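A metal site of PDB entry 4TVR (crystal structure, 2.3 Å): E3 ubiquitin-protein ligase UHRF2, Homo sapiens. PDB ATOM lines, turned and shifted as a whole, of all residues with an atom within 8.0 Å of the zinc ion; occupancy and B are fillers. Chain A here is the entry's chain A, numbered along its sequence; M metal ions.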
ATOM      1  N   HIS A 228     -12.643  -8.795  -4.113  1.00  0.00           N
ATOM      2  CA  HIS A 228     -14.085  -9.045  -4.145  1.00  0.00           C
ATOM      3  C   HIS A 228     -14.663  -9.350  -2.752  1.00  0.00           C
ATOM      4  O   HIS A 228     -15.888  -9.284  -2.559  1.00  0.00           O
ATOM      5  CB  HIS A 228     -14.405 -10.221  -5.089  1.00  0.00           C
ATOM      6  CG  HIS A 228     -14.286  -9.876  -6.544  1.00  0.00           C
ATOM      7  ND1 HIS A 228     -15.383  -9.656  -7.344  1.00  0.00           N
ATOM      8  CD2 HIS A 228     -13.203  -9.748  -7.342  1.00  0.00           C
ATOM      9  CE1 HIS A 228     -14.984  -9.384  -8.576  1.00  0.00           C
ATOM     10  NE2 HIS A 228     -13.659  -9.437  -8.605  1.00  0.00           N
ATOM     11  N   SER A 231     -14.190  -5.631  -0.407  1.00  0.00           N
ATOM     12  CA  SER A 231     -14.602  -4.441  -1.155  1.00  0.00           C
ATOM     13  C   SER A 231     -15.777  -4.786  -2.084  1.00  0.00           C
ATOM     14  O   SER A 231     -16.512  -5.747  -1.809  1.00  0.00           O
ATOM     15  CB  SER A 231     -13.420  -3.859  -1.932  1.00  0.00           C
ATOM     16  OG  SER A 231     -13.736  -2.598  -2.489  1.00  0.00           O
ATOM     17  N   CYS A 232     -15.963  -4.036  -3.172  1.00  0.00           N
ATOM     18  CA  CYS A 232     -17.101  -4.250  -4.072  1.00  0.00           C
ATOM     19  C   CYS A 232     -17.132  -5.695  -4.606  1.00  0.00           C
ATOM     20  O   CYS A 232     -16.153  -6.179  -5.161  1.00  0.00           O
ATOM     21  CB  CYS A 232     -17.078  -3.263  -5.239  1.00  0.00           C
ATOM     22  SG  CYS A 232     -18.325  -3.562  -6.521  1.00  0.00           S
ATOM     23  N   ARG A 233     -18.273  -6.352  -4.426  1.00  0.00           N
ATOM     24  CA  ARG A 233     -18.442  -7.757  -4.797  1.00  0.00           C
ATOM     25  C   ARG A 233     -18.474  -7.952  -6.308  1.00  0.00           C
ATOM     26  O   ARG A 233     -18.018  -8.980  -6.819  1.00  0.00           O
ATOM     27  CB  ARG A 233     -19.721  -8.314  -4.164  1.00  0.00           C
ATOM     28  CG  ARG A 233     -19.731  -9.827  -3.984  1.00  0.00           C
ATOM     29  CD  ARG A 233     -20.906 -10.254  -3.103  1.00  0.00           C
ATOM     30  NE  ARG A 233     -20.646 -11.464  -2.322  1.00  0.00           N
ATOM     31  CZ  ARG A 233     -19.811 -11.540  -1.277  1.00  0.00           C
ATOM     32  NH1 ARG A 233     -19.103 -10.481  -0.878  1.00  0.00           N
ATOM     33  NH2 ARG A 233     -19.664 -12.695  -0.639  1.00  0.00           N
ATOM     34  N   VAL A 234     -19.013  -6.963  -7.034  1.00  0.00           N
ATOM     35  CA  VAL A 234     -19.160  -7.061  -8.486  1.00  0.00           C
ATOM     36  C   VAL A 234     -17.849  -6.854  -9.241  1.00  0.00           C
ATOM     37  O   VAL A 234     -17.527  -7.628 -10.143  1.00  0.00           O
ATOM     38  CB  VAL A 234     -20.216  -6.053  -9.006  1.00  0.00           C
ATOM     39  CG1 VAL A 234     -20.346  -6.135 -10.520  1.00  0.00           C
ATOM     40  CG2 VAL A 234     -21.570  -6.310  -8.340  1.00  0.00           C
ATOM     41  N   CYS A 235     -17.095  -5.825  -8.870  1.00  0.00           N
ATOM     42  CA  CYS A 235     -15.870  -5.461  -9.598  1.00  0.00           C
ATOM     43  C   CYS A 235     -14.556  -5.600  -8.817  1.00  0.00           C
ATOM     44  O   CYS A 235     -13.495  -5.764  -9.426  1.00  0.00           O
ATOM     45  CB  CYS A 235     -15.996  -4.022 -10.152  1.00  0.00           C
ATOM     46  SG  CYS A 235     -15.832  -2.698  -8.928  1.00  0.00           S
ATOM     47  N   GLY A 236     -14.603  -5.523  -7.492  1.00  0.00           N
ATOM     48  CA  GLY A 236     -13.408  -5.646  -6.652  1.00  0.00           C
ATOM     49  C   GLY A 236     -12.528  -4.409  -6.711  1.00  0.00           C
ATOM     50  O   GLY A 236     -11.321  -4.501  -6.886  1.00  0.00           O
ATOM     51  N   GLY A 237     -13.152  -3.239  -6.551  1.00  0.00           N
ATOM     52  CA  GLY A 237     -12.459  -1.956  -6.604  1.00  0.00           C
ATOM     53  C   GLY A 237     -12.667  -1.157  -5.338  1.00  0.00           C
ATOM     54  O   GLY A 237     -13.799  -0.815  -4.982  1.00  0.00           O
ATOM     55  N   LYS A 238     -11.568  -0.860  -4.640  1.00  0.00           N
ATOM     56  CA  LYS A 238     -11.602  -0.063  -3.406  1.00  0.00           C
ATOM     57  C   LYS A 238     -11.697   1.438  -3.696  1.00  0.00           C
ATOM     58  O   LYS A 238     -11.915   2.232  -2.766  1.00  0.00           O
ATOM     59  CB  LYS A 238     -10.377  -0.360  -2.545  1.00  0.00           C
ATOM     60  CG  LYS A 238     -10.399  -1.741  -1.927  1.00  0.00           C
ATOM     61  CD  LYS A 238      -9.023  -2.173  -1.447  1.00  0.00           C
ATOM     62  CE  LYS A 238      -9.045  -3.614  -0.961  1.00  0.00           C
ATOM     63  NZ  LYS A 238      -7.672  -4.161  -0.764  1.00  0.00           N
ATOM     64  N   HIS A 239     -11.508   1.823  -4.953  1.00  0.00           N
ATOM     65  CA  HIS A 239     -11.690   3.209  -5.385  1.00  0.00           C
ATOM     66  C   HIS A 239     -13.087   3.717  -4.998  1.00  0.00           C
ATOM     67  O   HIS A 239     -14.064   2.970  -5.041  1.00  0.00           O
ATOM     68  CB  HIS A 239     -11.475   3.349  -6.903  1.00  0.00           C
ATOM     69  CG  HIS A 239     -12.486   2.633  -7.741  1.00  0.00           C
ATOM     70  ND1 HIS A 239     -12.324   1.323  -8.138  1.00  0.00           N
ATOM     71  CD2 HIS A 239     -13.662   3.037  -8.266  1.00  0.00           C
ATOM     72  CE1 HIS A 239     -13.363   0.952  -8.867  1.00  0.00           C
ATOM     73  NE2 HIS A 239     -14.192   1.981  -8.960  1.00  0.00           N
ATOM     74  N   GLU A 240     -13.144   4.993  -4.620  1.00  0.00           N
ATOM     75  CA  GLU A 240     -14.384   5.635  -4.173  1.00  0.00           C
ATOM     76  C   GLU A 240     -14.970   4.941  -2.937  1.00  0.00           C
ATOM     77  O   GLU A 240     -15.907   4.144  -3.043  1.00  0.00           O
ATOM     78  CB  GLU A 240     -15.432   5.677  -5.294  1.00  0.00           C
ATOM     79  CG  GLU A 240     -14.954   6.316  -6.588  1.00  0.00           C
ATOM     80  CD  GLU A 240     -15.956   6.185  -7.722  1.00  0.00           C
ATOM     81  OE1 GLU A 240     -17.127   5.834  -7.453  1.00  0.00           O
ATOM     82  OE2 GLU A 240     -15.565   6.429  -8.876  1.00  0.00           O
ATOM     83  N   MET A 243     -18.643   6.662  -2.904  1.00  0.00           N
ATOM     84  CA  MET A 243     -19.677   6.234  -3.860  1.00  0.00           C
ATOM     85  C   MET A 243     -19.858   4.723  -3.837  1.00  0.00           C
ATOM     86  O   MET A 243     -19.853   4.068  -4.890  1.00  0.00           O
ATOM     87  CB  MET A 243     -19.316   6.702  -5.274  1.00  0.00           C
ATOM     88  N   GLN A 244     -20.046   4.170  -2.637  1.00  0.00           N
ATOM     89  CA  GLN A 244     -20.082   2.725  -2.433  1.00  0.00           C
ATOM     90  C   GLN A 244     -20.666   2.413  -1.041  1.00  0.00           C
ATOM     91  O   GLN A 244     -20.028   2.694  -0.031  1.00  0.00           O
ATOM     92  CB  GLN A 244     -18.667   2.149  -2.568  1.00  0.00           C
ATOM     93  CG  GLN A 244     -18.521   0.654  -2.275  1.00  0.00           C
ATOM     94  CD  GLN A 244     -17.101   0.167  -2.492  1.00  0.00           C
ATOM     95  OE1 GLN A 244     -16.443   0.512  -3.468  1.00  0.00           O
ATOM     96  NE2 GLN A 244     -16.610  -0.662  -1.566  1.00  0.00           N
ATOM     97  N   ALA A 253     -20.067  -4.912   0.236  1.00  0.00           N
ATOM     98  CA  ALA A 253     -20.244  -3.626  -0.424  1.00  0.00           C
ATOM     99  C   ALA A 253     -20.640  -3.713  -1.901  1.00  0.00           C
ATOM    100  O   ALA A 253     -20.459  -4.749  -2.553  1.00  0.00           O
ATOM    101  CB  ALA A 253     -18.977  -2.782  -0.272  1.00  0.00           C
ATOM    102  N   TYR A 254     -21.180  -2.612  -2.417  1.00  0.00           N
ATOM    103  CA  TYR A 254     -21.523  -2.459  -3.838  1.00  0.00           C
ATOM    104  C   TYR A 254     -21.401  -0.984  -4.239  1.00  0.00           C
ATOM    105  O   TYR A 254     -21.776  -0.104  -3.457  1.00  0.00           O
ATOM    106  CB  TYR A 254     -22.964  -2.920  -4.096  1.00  0.00           C
ATOM    107  CG  TYR A 254     -23.190  -4.413  -4.081  1.00  0.00           C
ATOM    108  CD1 TYR A 254     -23.559  -5.066  -2.906  1.00  0.00           C
ATOM    109  CD2 TYR A 254     -23.058  -5.174  -5.239  1.00  0.00           C
ATOM    110  CE1 TYR A 254     -23.780  -6.438  -2.880  1.00  0.00           C
ATOM    111  CE2 TYR A 254     -23.266  -6.543  -5.225  1.00  0.00           C
ATOM    112  CZ  TYR A 254     -23.635  -7.169  -4.043  1.00  0.00           C
ATOM    113  OH  TYR A 254     -23.857  -8.525  -4.023  1.00  0.00           O
ATOM    114  N   HIS A 255     -20.873  -0.717  -5.433  1.00  0.00           N
ATOM    115  CA  HIS A 255     -20.857   0.649  -5.970  1.00  0.00           C
ATOM    116  C   HIS A 255     -22.267   1.054  -6.399  1.00  0.00           C
ATOM    117  O   HIS A 255     -23.128   0.189  -6.611  1.00  0.00           O
ATOM    118  CB  HIS A 255     -19.911   0.779  -7.173  1.00  0.00           C
ATOM    119  CG  HIS A 255     -18.461   0.739  -6.822  1.00  0.00           C
ATOM    120  ND1 HIS A 255     -17.657  -0.347  -7.087  1.00  0.00           N
ATOM    121  CD2 HIS A 255     -17.651   1.665  -6.236  1.00  0.00           C
ATOM    122  CE1 HIS A 255     -16.428  -0.098  -6.679  1.00  0.00           C
ATOM    123  NE2 HIS A 255     -16.394   1.118  -6.165  1.00  0.00           N
ATOM    124  N   ILE A 256     -22.508   2.359  -6.526  1.00  0.00           N
ATOM    125  CA  ILE A 256     -23.794   2.882  -6.966  1.00  0.00           C
ATOM    126  C   ILE A 256     -24.136   2.452  -8.398  1.00  0.00           C
ATOM    127  O   ILE A 256     -25.301   2.304  -8.749  1.00  0.00           O
ATOM    128  CB  ILE A 256     -23.834   4.424  -6.897  1.00  0.00           C
ATOM    129  N   TYR A 257     -23.095   2.240  -9.207  1.00  0.00           N
ATOM    130  CA  TYR A 257     -23.257   1.870 -10.625  1.00  0.00           C
ATOM    131  C   TYR A 257     -22.962   0.387 -10.904  1.00  0.00           C
ATOM    132  O   TYR A 257     -22.976  -0.026 -12.066  1.00  0.00           O
ATOM    133  CB  TYR A 257     -22.377   2.779 -11.510  1.00  0.00           C
ATOM    134  CG  TYR A 257     -20.964   2.990 -10.999  1.00  0.00           C
ATOM    135  CD1 TYR A 257     -19.980   2.016 -11.204  1.00  0.00           C
ATOM    136  CD2 TYR A 257     -20.604   4.148 -10.319  1.00  0.00           C
ATOM    137  CE1 TYR A 257     -18.689   2.198 -10.741  1.00  0.00           C
ATOM    138  CE2 TYR A 257     -19.313   4.343  -9.853  1.00  0.00           C
ATOM    139  CZ  TYR A 257     -18.352   3.365 -10.065  1.00  0.00           C
ATOM    140  OH  TYR A 257     -17.075   3.546  -9.600  1.00  0.00           O
ATOM    141  N   CYS A 258     -22.710  -0.396  -9.858  1.00  0.00           N
ATOM    142  CA  CYS A 258     -22.421  -1.840 -10.010  1.00  0.00           C
ATOM    143  C   CYS A 258     -23.608  -2.749  -9.679  1.00  0.00           C
ATOM    144  O   CYS A 258     -23.593  -3.929 -10.034  1.00  0.00           O
ATOM    145  CB  CYS A 258     -21.228  -2.249  -9.142  1.00  0.00           C
ATOM    146  SG  CYS A 258     -19.619  -1.928  -9.901  1.00  0.00           S
ATOM    147  N   LEU A 259     -24.625  -2.208  -9.006  1.00  0.00           N
ATOM    148  CA  LEU A 259     -25.828  -2.970  -8.706  1.00  0.00           C
ATOM    149  C   LEU A 259     -26.615  -3.263  -9.987  1.00  0.00           C
ATOM    150  O   LEU A 259     -26.462  -2.550 -10.990  1.00  0.00           O
ATOM    151  CB  LEU A 259     -26.716  -2.216  -7.715  1.00  0.00           C
ATOM    152  CG  LEU A 259     -26.143  -2.017  -6.314  1.00  0.00           C
ATOM    153  CD1 LEU A 259     -26.942  -0.978  -5.547  1.00  0.00           C
ATOM    154  CD2 LEU A 259     -26.113  -3.335  -5.552  1.00  0.00           C
HETATM  155 ZN    ZN M   1     -17.973  -2.034  -8.256  1.00  0.00          ZN
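The nearest printed residue that does not touch the zinc ion is Val 234 (4.7 Å).
The zinc ion is bound by ND1 of His 255, at 2.1 Å. The zinc ion is bound by SG of Cys 258 (2.3 Å). SG of Cys 232 is bound to the zinc ion (2.3 Å). SG of Cys 235 is bound to the zinc ion (2.3 Å).
The side-chain sulfur (SG) of Cys 232 sits close to the backbone NH (N) of Val 234 (3.5 Å). The side-chain sulfur (SG) of Cys 235 lies close to the backbone NH (N) of Gly 237 (3.6 Å). The backbone carbonyl oxygen (O) of Gly 237 sits close to a ring nitrogen (NE2) of His 255. The backbone carbonyl oxygen of His 239 sits at hydrogen-bond distance from a ring nitrogen (NE2) of His 255 (3.2 Å). NE2 of His 255 lies within hydrogen-bond range of OE1 of Gln 244 (2.8 Å).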
